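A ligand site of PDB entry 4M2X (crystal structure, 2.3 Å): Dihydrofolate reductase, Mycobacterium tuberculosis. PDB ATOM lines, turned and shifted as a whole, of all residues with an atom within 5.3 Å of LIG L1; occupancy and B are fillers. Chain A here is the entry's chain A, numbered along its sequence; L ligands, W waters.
N1 of LIG L1 sits at hydrogen-bond distance from OD2 of Asp 30, 2.6 Å away.
N5 of LIG L1 sits close to O of Ile 97, at 2.9 Å.
The backbone carbonyl oxygen of Ile 8 sits at hydrogen-bond distance from a nitrogen (N5) of LIG L1 (2.9 Å).
The backbone NH of Trp 9 lies close to a nitrogen (N2) of LIG L1 (3.4 Å).
N4 of LIG L1 sits close to O of Trp 9, at 3.4 Å.
OG1 of Thr 116 is in hydrogen-bond range of N4 of LIG L1, at 3.4 Å.
OH of Tyr 103 sits at hydrogen-bond distance from N5 of LIG L1, 3.4 Å away.
The backbone NH of Ala 10 sits at hydrogen-bond distance from an oxygen (O14) of LG2 L2, 2.8 Å away.
The backbone carbonyl oxygen of Ala 10 lies within hydrogen-bond range of a nitrogen (N7) of LG2 L2 (2.7 Å).
O12 of LG2 L2 is in hydrogen-bond range of N of Asp 22.
O12 of LG2 L2 lies within hydrogen-bond range of O of Asp 22, 3.3 Å away.
The backbone NH (N) of Thr 49 lies within hydrogen-bond range of an oxygen (O2) of LG2 L2, at 3.3 Å.
The side-chain hydroxyl (OG1) of Thr 49 lies within hydrogen-bond range of an oxygen (O2) of LG2 L2, at 2.7 Å.
OD1 of Asp 30 sits at hydrogen-bond distance from OG1 of Thr 116 (2.7 Å).
The side-chain hydroxyl (OH) of Tyr 103 is in hydrogen-bond range of the backbone carbonyl oxygen (O) of Ile 97 (3.1 Å).
O of Ile 8 is in hydrogen-bond range of OH of Tyr 103, 2.5 Å away.
The backbone NH (N) of Ile 8 is in hydrogen-bond range of the backbone carbonyl oxygen (O) of Val 96, at 3.0 Å.
The backbone carbonyl oxygen of Trp 9 is in hydrogen-bond range of the backbone NH of Thr 116 (2.9 Å).
The backbone NH (N) of Trp 9 sits at hydrogen-bond distance from the backbone carbonyl oxygen (O) of Glu 114, 2.9 Å away.
O of Ile 23 lies within hydrogen-bond range of NH1 of Arg 26.
The guanidinium group (NH2) of Arg 26 lies within salt-bridge range of the side-chain carboxylate (OD2) of Asp 22 (3.2 Å).
Merely in contact with LIG L1: Ala 10 (3.5 Å), Asp 22 (3.97 Å), Ile 23 (3.3 Å), Arg 26 (3.2 Å), Gln 31 (2.9 Å), Phe 34 (3.3 Å), Leu 53 (3.7 Å), Pro 54 (3.2 Å) and Leu 60 (3.9 Å).
Hydrophobic or aromatic side chains within 4 Å of LIG L1: Ile 8, Ala 10, Ile 23, Phe 34, Leu 53, Pro 54, Leu 60 and Ile 97.
15 residues have an atom within 4 Å of LIG L1: Ile 8, Trp 9, Ala 10, Asp 22, Ile 23, Arg 26, Asp 30, Gln 31, Phe 34, Leu 53, Pro 54, Leu 60, Ile 97, Tyr 103 and Thr 116.
Water W2 lies within hydrogen-bond range of the side-chain hydroxyl of Ser 52, an oxygen (O13) of LG2 L2 and a nitrogen (N3) of LIG L1.
Water W1 lies within hydrogen-bond range of N4 of LIG L1 (2.8 Å), OG1 of Thr 116 (2.8 Å), O of Glu 114 (3.1 Å), O of Trp 9 (3.4 Å) and ND1 of His 33 (3.4 Å).
Water W3 bridges OD2 of Asp 22 and O of Ser 52.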
ATOM      1  N   ILE A   8      -3.371  -9.455  -0.253  1.00  0.00           N
ATOM      2  CA  ILE A   8      -2.506  -8.355  -0.653  1.00  0.00           C
ATOM      3  C   ILE A   8      -3.366  -7.159  -1.035  1.00  0.00           C
ATOM      4  O   ILE A   8      -4.318  -7.282  -1.794  1.00  0.00           O
ATOM      5  CB  ILE A   8      -1.625  -8.752  -1.855  1.00  0.00           C
ATOM      6  CG1 ILE A   8      -0.655  -7.625  -2.217  1.00  0.00           C
ATOM      7  CG2 ILE A   8      -2.455  -9.150  -3.063  1.00  0.00           C
ATOM      8  CD1 ILE A   8       0.509  -8.112  -3.125  1.00  0.00           C
ATOM      9  N   TRP A   9      -3.003  -5.992  -0.514  1.00  0.00           N
ATOM     10  CA  TRP A   9      -3.694  -4.770  -0.860  1.00  0.00           C
ATOM     11  C   TRP A   9      -2.828  -3.549  -0.598  1.00  0.00           C
ATOM     12  O   TRP A   9      -1.810  -3.620   0.079  1.00  0.00           O
ATOM     13  CB  TRP A   9      -4.969  -4.621  -0.012  1.00  0.00           C
ATOM     14  CG  TRP A   9      -4.713  -4.272   1.416  1.00  0.00           C
ATOM     15  CD1 TRP A   9      -4.483  -3.034   1.923  1.00  0.00           C
ATOM     16  CD2 TRP A   9      -4.683  -5.172   2.543  1.00  0.00           C
ATOM     17  NE1 TRP A   9      -4.321  -3.098   3.291  1.00  0.00           N
ATOM     18  CE2 TRP A   9      -4.434  -4.412   3.688  1.00  0.00           C
ATOM     19  CE3 TRP A   9      -4.847  -6.560   2.678  1.00  0.00           C
ATOM     20  CZ2 TRP A   9      -4.333  -4.969   4.953  1.00  0.00           C
ATOM     21  CZ3 TRP A   9      -4.736  -7.117   3.911  1.00  0.00           C
ATOM     22  CH2 TRP A   9      -4.483  -6.330   5.042  1.00  0.00           C
ATOM     23  N   ALA A  10      -3.293  -2.431  -1.134  1.00  0.00           N
ATOM     24  CA  ALA A  10      -2.668  -1.142  -0.931  1.00  0.00           C
ATOM     25  C   ALA A  10      -3.696  -0.260  -0.265  1.00  0.00           C
ATOM     26  O   ALA A  10      -4.828  -0.177  -0.736  1.00  0.00           O
ATOM     27  CB  ALA A  10      -2.221  -0.550  -2.256  1.00  0.00           C
ATOM     28  N   ASP A  22     -13.056   2.718  -7.528  1.00  0.00           N
ATOM     29  CA  ASP A  22     -11.716   2.973  -8.025  1.00  0.00           C
ATOM     30  C   ASP A  22     -10.815   3.150  -6.826  1.00  0.00           C
ATOM     31  O   ASP A  22     -11.275   3.137  -5.690  1.00  0.00           O
ATOM     32  CB  ASP A  22     -11.701   4.253  -8.853  1.00  0.00           C
ATOM     33  CG  ASP A  22     -10.542   4.319  -9.847  1.00  0.00           C
ATOM     34  OD1 ASP A  22     -10.579   5.241 -10.684  1.00  0.00           O
ATOM     35  OD2 ASP A  22      -9.617   3.460  -9.810  1.00  0.00           O
ATOM     36  N   ILE A  23      -9.537   3.309  -7.090  1.00  0.00           N
ATOM     37  CA  ILE A  23      -8.572   3.476  -6.042  1.00  0.00           C
ATOM     38  C   ILE A  23      -8.197   4.947  -6.036  1.00  0.00           C
ATOM     39  O   ILE A  23      -7.945   5.517  -7.087  1.00  0.00           O
ATOM     40  CB  ILE A  23      -7.356   2.587  -6.314  1.00  0.00           C
ATOM     41  CG1 ILE A  23      -7.814   1.132  -6.301  1.00  0.00           C
ATOM     42  CG2 ILE A  23      -6.282   2.843  -5.282  1.00  0.00           C
ATOM     43  CD1 ILE A  23      -6.758   0.160  -6.661  1.00  0.00           C
ATOM     44  N   ARG A  26      -2.600   6.791  -7.525  1.00  0.00           N
ATOM     45  CA  ARG A  26      -1.867   6.012  -8.517  1.00  0.00           C
ATOM     46  C   ARG A  26      -0.451   5.893  -8.021  1.00  0.00           C
ATOM     47  O   ARG A  26       0.232   6.886  -7.798  1.00  0.00           O
ATOM     48  CB  ARG A  26      -1.895   6.661  -9.889  1.00  0.00           C
ATOM     49  CG  ARG A  26      -3.264   6.635 -10.545  1.00  0.00           C
ATOM     50  CD  ARG A  26      -3.800   5.225 -10.655  1.00  0.00           C
ATOM     51  NE  ARG A  26      -5.106   5.209 -11.310  1.00  0.00           N
ATOM     52  CZ  ARG A  26      -6.266   5.102 -10.673  1.00  0.00           C
ATOM     53  NH1 ARG A  26      -6.309   4.975  -9.357  1.00  0.00           N
ATOM     54  NH2 ARG A  26      -7.392   5.097 -11.368  1.00  0.00           N
ATOM     55  N   ASP A  30       3.595   0.460  -6.524  1.00  0.00           N
ATOM     56  CA  ASP A  30       2.693  -0.504  -5.909  1.00  0.00           C
ATOM     57  C   ASP A  30       2.174  -1.545  -6.915  1.00  0.00           C
ATOM     58  O   ASP A  30       2.107  -2.731  -6.607  1.00  0.00           O
ATOM     59  CB  ASP A  30       1.526   0.195  -5.204  1.00  0.00           C
ATOM     60  CG  ASP A  30       0.459  -0.788  -4.736  1.00  0.00           C
ATOM     61  OD1 ASP A  30       0.795  -1.671  -3.903  1.00  0.00           O
ATOM     62  OD2 ASP A  30      -0.688  -0.690  -5.215  1.00  0.00           O
ATOM     63  N   GLN A  31       1.815  -1.092  -8.115  1.00  0.00           N
ATOM     64  CA  GLN A  31       1.437  -2.009  -9.205  1.00  0.00           C
ATOM     65  C   GLN A  31       2.532  -3.057  -9.416  1.00  0.00           C
ATOM     66  O   GLN A  31       2.251  -4.252  -9.542  1.00  0.00           O
ATOM     67  CB  GLN A  31       1.207  -1.252 -10.513  1.00  0.00           C
ATOM     68  CG  GLN A  31       0.179  -0.144 -10.412  1.00  0.00           C
ATOM     69  CD  GLN A  31       0.082   0.669 -11.675  1.00  0.00           C
ATOM     70  OE1 GLN A  31       0.039   0.125 -12.782  1.00  0.00           O
ATOM     71  NE2 GLN A  31       0.033   1.979 -11.530  1.00  0.00           N
ATOM     72  N   HIS A  33       4.920  -3.992  -7.305  1.00  0.00           N
ATOM     73  CA  HIS A  33       4.893  -4.895  -6.169  1.00  0.00           C
ATOM     74  C   HIS A  33       3.768  -5.922  -6.249  1.00  0.00           C
ATOM     75  O   HIS A  33       3.969  -7.093  -5.964  1.00  0.00           O
ATOM     76  CB  HIS A  33       4.726  -4.116  -4.881  1.00  0.00           C
ATOM     77  CG  HIS A  33       5.050  -4.912  -3.672  1.00  0.00           C
ATOM     78  ND1 HIS A  33       4.135  -5.156  -2.668  1.00  0.00           N
ATOM     79  CD2 HIS A  33       6.188  -5.556  -3.300  1.00  0.00           C
ATOM     80  CE1 HIS A  33       4.702  -5.898  -1.737  1.00  0.00           C
ATOM     81  NE2 HIS A  33       5.946  -6.151  -2.093  1.00  0.00           N
ATOM     82  N   PHE A  34       2.582  -5.455  -6.601  1.00  0.00           N
ATOM     83  CA  PHE A  34       1.417  -6.335  -6.674  1.00  0.00           C
ATOM     84  C   PHE A  34       1.678  -7.409  -7.742  1.00  0.00           C
ATOM     85  O   PHE A  34       1.477  -8.605  -7.516  1.00  0.00           O
ATOM     86  CB  PHE A  34       0.166  -5.517  -6.994  1.00  0.00           C
ATOM     87  CG  PHE A  34      -1.008  -6.334  -7.446  1.00  0.00           C
ATOM     88  CD1 PHE A  34      -1.748  -7.065  -6.542  1.00  0.00           C
ATOM     89  CD2 PHE A  34      -1.369  -6.365  -8.777  1.00  0.00           C
ATOM     90  CE1 PHE A  34      -2.810  -7.805  -6.946  1.00  0.00           C
ATOM     91  CE2 PHE A  34      -2.440  -7.112  -9.190  1.00  0.00           C
ATOM     92  CZ  PHE A  34      -3.165  -7.824  -8.282  1.00  0.00           C
ATOM     93  N   THR A  49     -14.125  -5.725  -7.851  1.00  0.00           N
ATOM     94  CA  THR A  49     -12.715  -5.493  -8.171  1.00  0.00           C
ATOM     95  C   THR A  49     -12.522  -5.769  -9.644  1.00  0.00           C
ATOM     96  O   THR A  49     -11.983  -4.936 -10.378  1.00  0.00           O
ATOM     97  CB  THR A  49     -11.813  -6.368  -7.328  1.00  0.00           C
ATOM     98  OG1 THR A  49     -11.941  -5.966  -5.971  1.00  0.00           O
ATOM     99  CG2 THR A  49     -10.329  -6.237  -7.756  1.00  0.00           C
ATOM    100  N   SER A  52     -13.727  -3.091 -11.537  1.00  0.00           N
ATOM    101  CA  SER A  52     -12.839  -1.944 -11.337  1.00  0.00           C
ATOM    102  C   SER A  52     -11.539  -2.015 -12.137  1.00  0.00           C
ATOM    103  O   SER A  52     -10.847  -1.005 -12.283  1.00  0.00           O
ATOM    104  CB  SER A  52     -12.504  -1.756  -9.852  1.00  0.00           C
ATOM    105  OG  SER A  52     -11.460  -2.623  -9.448  1.00  0.00           O
ATOM    106  N   LEU A  53     -11.195  -3.195 -12.626  1.00  0.00           N
ATOM    107  CA  LEU A  53      -9.963  -3.365 -13.383  1.00  0.00           C
ATOM    108  C   LEU A  53     -10.068  -2.679 -14.737  1.00  0.00           C
ATOM    109  O   LEU A  53     -11.002  -2.938 -15.503  1.00  0.00           O
ATOM    110  CB  LEU A  53      -9.653  -4.847 -13.596  1.00  0.00           C
ATOM    111  CG  LEU A  53      -9.303  -5.692 -12.370  1.00  0.00           C
ATOM    112  CD1 LEU A  53      -9.078  -7.153 -12.813  1.00  0.00           C
ATOM    113  CD2 LEU A  53      -8.065  -5.136 -11.644  1.00  0.00           C
ATOM    114  N   PRO A  54      -9.089  -1.843 -15.062  1.00  0.00           N
ATOM    115  CA  PRO A  54      -9.046  -1.297 -16.415  1.00  0.00           C
ATOM    116  C   PRO A  54      -9.091  -2.461 -17.398  1.00  0.00           C
ATOM    117  O   PRO A  54      -8.440  -3.481 -17.170  1.00  0.00           O
ATOM    118  CB  PRO A  54      -7.690  -0.593 -16.453  1.00  0.00           C
ATOM    119  CG  PRO A  54      -7.398  -0.254 -15.028  1.00  0.00           C
ATOM    120  CD  PRO A  54      -7.947  -1.405 -14.241  1.00  0.00           C
ATOM    121  N   VAL A  57      -6.082  -4.857 -18.407  1.00  0.00           N
ATOM    122  CA  VAL A  57      -5.433  -5.753 -17.439  1.00  0.00           C
ATOM    123  C   VAL A  57      -6.433  -6.702 -16.802  1.00  0.00           C
ATOM    124  O   VAL A  57      -6.250  -7.126 -15.677  1.00  0.00           O
ATOM    125  CB  VAL A  57      -4.706  -5.006 -16.308  1.00  0.00           C
ATOM    126  CG1 VAL A  57      -3.604  -4.134 -16.853  1.00  0.00           C
ATOM    127  CG2 VAL A  57      -5.684  -4.176 -15.502  1.00  0.00           C
ATOM    128  N   LEU A  60      -6.168 -10.412 -15.188  1.00  0.00           N
ATOM    129  CA  LEU A  60      -4.776 -10.079 -14.881  1.00  0.00           C
ATOM    130  C   LEU A  60      -3.812 -11.072 -15.531  1.00  0.00           C
ATOM    131  O   LEU A  60      -3.816 -12.267 -15.229  1.00  0.00           O
ATOM    132  CB  LEU A  60      -4.534 -10.003 -13.376  1.00  0.00           C
ATOM    133  CG  LEU A  60      -5.121  -8.744 -12.773  1.00  0.00           C
ATOM    134  CD1 LEU A  60      -5.199  -8.867 -11.260  1.00  0.00           C
ATOM    135  CD2 LEU A  60      -4.349  -7.501 -13.182  1.00  0.00           C
ATOM    136  N   VAL A  96      -5.498 -13.477  -2.441  1.00  0.00           N
ATOM    137  CA  VAL A  96      -6.727 -12.705  -2.431  1.00  0.00           C
ATOM    138  C   VAL A  96      -6.340 -11.256  -2.686  1.00  0.00           C
ATOM    139  O   VAL A  96      -5.620 -10.649  -1.872  1.00  0.00           O
ATOM    140  CB  VAL A  96      -7.450 -12.838  -1.067  1.00  0.00           C
ATOM    141  CG1 VAL A  96      -8.672 -11.934  -0.980  1.00  0.00           C
ATOM    142  CG2 VAL A  96      -7.815 -14.288  -0.809  1.00  0.00           C
ATOM    143  N   ILE A  97      -6.800 -10.691  -3.807  1.00  0.00           N
ATOM    144  CA  ILE A  97      -6.380  -9.341  -4.202  1.00  0.00           C
ATOM    145  C   ILE A  97      -7.524  -8.346  -4.193  1.00  0.00           C
ATOM    146  O   ILE A  97      -7.407  -7.234  -4.711  1.00  0.00           O
ATOM    147  CB  ILE A  97      -5.858  -9.344  -5.652  1.00  0.00           C
ATOM    148  CG1 ILE A  97      -7.035  -9.279  -6.625  1.00  0.00           C
ATOM    149  CG2 ILE A  97      -5.074 -10.600  -5.889  1.00  0.00           C
ATOM    150  CD1 ILE A  97      -6.652  -9.194  -8.073  1.00  0.00           C
ATOM    151  N   GLY A  98      -8.631  -8.745  -3.603  1.00  0.00           N
ATOM    152  CA  GLY A  98      -9.867  -8.424  -4.283  1.00  0.00           C
ATOM    153  C   GLY A  98     -11.065  -7.888  -3.595  1.00  0.00           C
ATOM    154  O   GLY A  98     -12.091  -8.500  -3.623  1.00  0.00           O
ATOM    155  N   TYR A 103     -11.673  -9.308   1.300  1.00  0.00           N
ATOM    156  CA  TYR A 103     -10.617  -9.487   2.298  1.00  0.00           C
ATOM    157  C   TYR A 103     -11.251  -9.998   3.584  1.00  0.00           C
ATOM    158  O   TYR A 103     -10.750 -10.927   4.214  1.00  0.00           O
ATOM    159  CB  TYR A 103      -9.854  -8.189   2.558  1.00  0.00           C
ATOM    160  CG  TYR A 103      -8.987  -7.733   1.381  1.00  0.00           C
ATOM    161  CD1 TYR A 103      -9.077  -6.432   0.913  1.00  0.00           C
ATOM    162  CD2 TYR A 103      -8.096  -8.587   0.763  1.00  0.00           C
ATOM    163  CE1 TYR A 103      -8.319  -5.991  -0.130  1.00  0.00           C
ATOM    164  CE2 TYR A 103      -7.326  -8.159  -0.302  1.00  0.00           C
ATOM    165  CZ  TYR A 103      -7.439  -6.860  -0.736  1.00  0.00           C
ATOM    166  OH  TYR A 103      -6.704  -6.393  -1.789  1.00  0.00           O
ATOM    167  N   GLU A 114       0.218  -8.929   2.321  1.00  0.00           N
ATOM    168  CA  GLU A 114       1.173  -7.960   1.866  1.00  0.00           C
ATOM    169  C   GLU A 114       0.421  -6.647   1.715  1.00  0.00           C
ATOM    170  O   GLU A 114      -0.540  -6.544   0.949  1.00  0.00           O
ATOM    171  CB  GLU A 114       1.851  -8.395   0.545  1.00  0.00           C
ATOM    172  CG  GLU A 114       2.674  -9.674   0.659  1.00  0.00           C
ATOM    173  CD  GLU A 114       3.885  -9.518   1.579  1.00  0.00           C
ATOM    174  OE1 GLU A 114       4.386  -8.377   1.725  1.00  0.00           O
ATOM    175  OE2 GLU A 114       4.329 -10.549   2.141  1.00  0.00           O
ATOM    176  N   THR A 116       0.604  -2.437   1.164  1.00  0.00           N
ATOM    177  CA  THR A 116       1.310  -1.235   0.782  1.00  0.00           C
ATOM    178  C   THR A 116       0.560  -0.127   1.455  1.00  0.00           C
ATOM    179  O   THR A 116      -0.637   0.037   1.237  1.00  0.00           O
ATOM    180  CB  THR A 116       1.241  -1.013  -0.733  1.00  0.00           C
ATOM    181  OG1 THR A 116       1.771  -2.160  -1.407  1.00  0.00           O
ATOM    182  CG2 THR A 116       2.016   0.244  -1.121  1.00  0.00           C
HETATM  183  N1  LIG L   1      -2.064  -2.894  -4.916  1.00  0.00           N
HETATM  184  C1  LIG L   1      -1.779  -3.961  -3.899  1.00  0.00           C
HETATM  185  N2  LIG L   1      -2.672  -5.181  -3.812  1.00  0.00           N
HETATM  186  C2  LIG L   1      -3.806  -5.330  -4.696  1.00  0.00           C
HETATM  187  C3  LIG L   1      -3.196  -3.031  -5.834  1.00  0.00           C
HETATM  188  C4  LIG L   1      -4.091  -4.236  -5.757  1.00  0.00           C
HETATM  189  C5  LIG L   1      -5.307  -4.375  -6.754  1.00  0.00           C
HETATM  190  C6  LIG L   1      -5.559  -3.262  -7.783  1.00  0.00           C
HETATM  191  C7  LIG L   1      -4.650  -2.038  -7.855  1.00  0.00           C
HETATM  192  C8  LIG L   1      -3.452  -1.899  -6.886  1.00  0.00           C
HETATM  193  C9  LIG L   1      -6.761  -3.366  -8.730  1.00  0.00           C
HETATM  194  N3  LIG L   1      -6.989  -2.114  -9.324  1.00  0.00           N
HETATM  195  C10 LIG L   1      -6.168  -1.683 -10.427  1.00  0.00           C
HETATM  196  C11 LIG L   1      -6.379  -0.317 -11.072  1.00  0.00           C
HETATM  197  C12 LIG L   1      -5.480   0.141 -12.223  1.00  0.00           C
HETATM  198  C13 LIG L   1      -4.358  -0.791 -12.755  1.00  0.00           C
HETATM  199  C14 LIG L   1      -4.158  -2.163 -12.094  1.00  0.00           C
HETATM  200  C15 LIG L   1      -5.057  -2.611 -10.939  1.00  0.00           C
HETATM  201  C16 LIG L   1      -6.209  -5.622  -6.737  1.00  0.00           C
HETATM  202  O1  LIG L   1      -5.734   1.396 -12.796  1.00  0.00           O
HETATM  203  O2  LIG L   1      -3.520  -0.401 -13.807  1.00  0.00           O
HETATM  204  O3  LIG L   1      -3.169  -3.049 -12.541  1.00  0.00           O
HETATM  205  C17 LIG L   1      -6.833   2.120 -12.307  1.00  0.00           C
HETATM  206  C18 LIG L   1      -2.286  -1.046 -13.992  1.00  0.00           C
HETATM  207  C19 LIG L   1      -2.872  -4.165 -11.742  1.00  0.00           C
HETATM  208  N4  LIG L   1      -0.612  -3.855  -3.044  1.00  0.00           N
HETATM  209  N5  LIG L   1      -4.659  -6.459  -4.507  1.00  0.00           N
HETATM  210  P1  LG2 L   2     -15.358  -6.473  -3.721  1.00  0.00           P
HETATM  211  O1  LG2 L   2     -14.974  -7.059  -2.246  1.00  0.00           O
HETATM  212  O2  LG2 L   2     -14.257  -6.469  -4.690  1.00  0.00           O
HETATM  213  O3  LG2 L   2     -16.536  -7.408  -4.375  1.00  0.00           O
HETATM  214  C1  LG2 L   2     -17.850  -7.220  -3.925  1.00  0.00           C
HETATM  215  C2  LG2 L   2     -18.599  -8.302  -4.718  1.00  0.00           C
HETATM  216  O4  LG2 L   2     -17.940  -9.561  -4.449  1.00  0.00           O
HETATM  217  C3  LG2 L   2     -20.033  -8.489  -4.257  1.00  0.00           C
HETATM  218  O5  LG2 L   2     -20.791  -7.572  -4.987  1.00  0.00           O
HETATM  219  C4  LG2 L   2     -20.303  -9.899  -4.700  1.00  0.00           C
HETATM  220  O6  LG2 L   2     -20.394  -9.983  -6.102  1.00  0.00           O
HETATM  221  C5  LG2 L   2     -18.963 -10.576  -4.419  1.00  0.00           C
HETATM  222  N1  LG2 L   2     -18.948 -11.234  -3.139  1.00  0.00           N
HETATM  223  C6  LG2 L   2     -18.966 -10.558  -1.837  1.00  0.00           C
HETATM  224  N2  LG2 L   2     -18.791 -11.605  -0.870  1.00  0.00           N
HETATM  225  C7  LG2 L   2     -19.331 -12.833  -1.446  1.00  0.00           C
HETATM  226  C8  LG2 L   2     -19.756 -14.158  -0.888  1.00  0.00           C
HETATM  227  N3  LG2 L   2     -19.692 -14.372   0.547  1.00  0.00           N
HETATM  228  N4  LG2 L   2     -20.248 -15.192  -1.766  1.00  0.00           N
HETATM  229  C9  LG2 L   2     -20.350 -14.936  -3.255  1.00  0.00           C
HETATM  230  N5  LG2 L   2     -19.933 -13.619  -3.823  1.00  0.00           N
HETATM  231  C10 LG2 L   2     -19.439 -12.589  -2.931  1.00  0.00           C
HETATM  232  O7  LG2 L   2     -16.154  -5.050  -3.618  1.00  0.00           O
HETATM  233  P2  LG2 L   2     -15.538  -3.832  -2.723  1.00  0.00           P
HETATM  234  O8  LG2 L   2     -16.431  -2.484  -3.052  1.00  0.00           O
HETATM  235  O9  LG2 L   2     -15.514  -4.189  -1.304  1.00  0.00           O
HETATM  236  O10 LG2 L   2     -14.015  -3.614  -3.302  1.00  0.00           O
HETATM  237  C11 LG2 L   2     -13.844  -3.061  -4.567  1.00  0.00           C
HETATM  238  C12 LG2 L   2     -13.201  -1.700  -4.271  1.00  0.00           C
HETATM  239  O11 LG2 L   2     -11.857  -1.888  -3.697  1.00  0.00           O
HETATM  240  C13 LG2 L   2     -13.030  -0.929  -5.578  1.00  0.00           C
HETATM  241  O12 LG2 L   2     -13.116   0.417  -5.238  1.00  0.00           O
HETATM  242  C14 LG2 L   2     -11.619  -1.214  -5.972  1.00  0.00           C
HETATM  243  O13 LG2 L   2     -11.115  -0.197  -6.801  1.00  0.00           O
HETATM  244  C15 LG2 L   2     -10.928  -1.263  -4.609  1.00  0.00           C
HETATM  245  N6  LG2 L   2      -9.687  -2.002  -4.624  1.00  0.00           N
HETATM  246  C16 LG2 L   2      -8.350  -1.508  -4.317  1.00  0.00           C
HETATM  247  C17 LG2 L   2      -7.630  -2.536  -3.485  1.00  0.00           C
HETATM  248  C18 LG2 L   2      -6.231  -1.972  -3.315  1.00  0.00           C
HETATM  249  O14 LG2 L   2      -5.382  -2.699  -2.935  1.00  0.00           O
HETATM  250  N7  LG2 L   2      -6.092  -0.533  -3.122  1.00  0.00           N
HETATM  251  C19 LG2 L   2      -7.602  -3.889  -4.214  1.00  0.00           C
HETATM  252  C20 LG2 L   2      -8.887  -4.345  -4.890  1.00  0.00           C
HETATM  253  C21 LG2 L   2      -9.871  -3.269  -5.318  1.00  0.00           C
HETATM  254  P3  LG2 L   2     -21.811  -9.730  -6.907  1.00  0.00           P
HETATM  255  O15 LG2 L   2     -22.346  -8.233  -6.523  1.00  0.00           O
HETATM  256  O16 LG2 L   2     -21.556  -9.792  -8.533  1.00  0.00           O
HETATM  257  O17 LG2 L   2     -22.725 -10.792  -6.493  1.00  0.00           O
HETATM  258  O   HOH W   1       1.078  -4.870  -1.122  1.00  0.00           O
HETATM  259  O   HOH W   2      -9.405  -1.009  -8.740  1.00  0.00           O
HETATM  260  O   HOH W   3      -9.304   1.174 -10.592  1.00  0.00           O
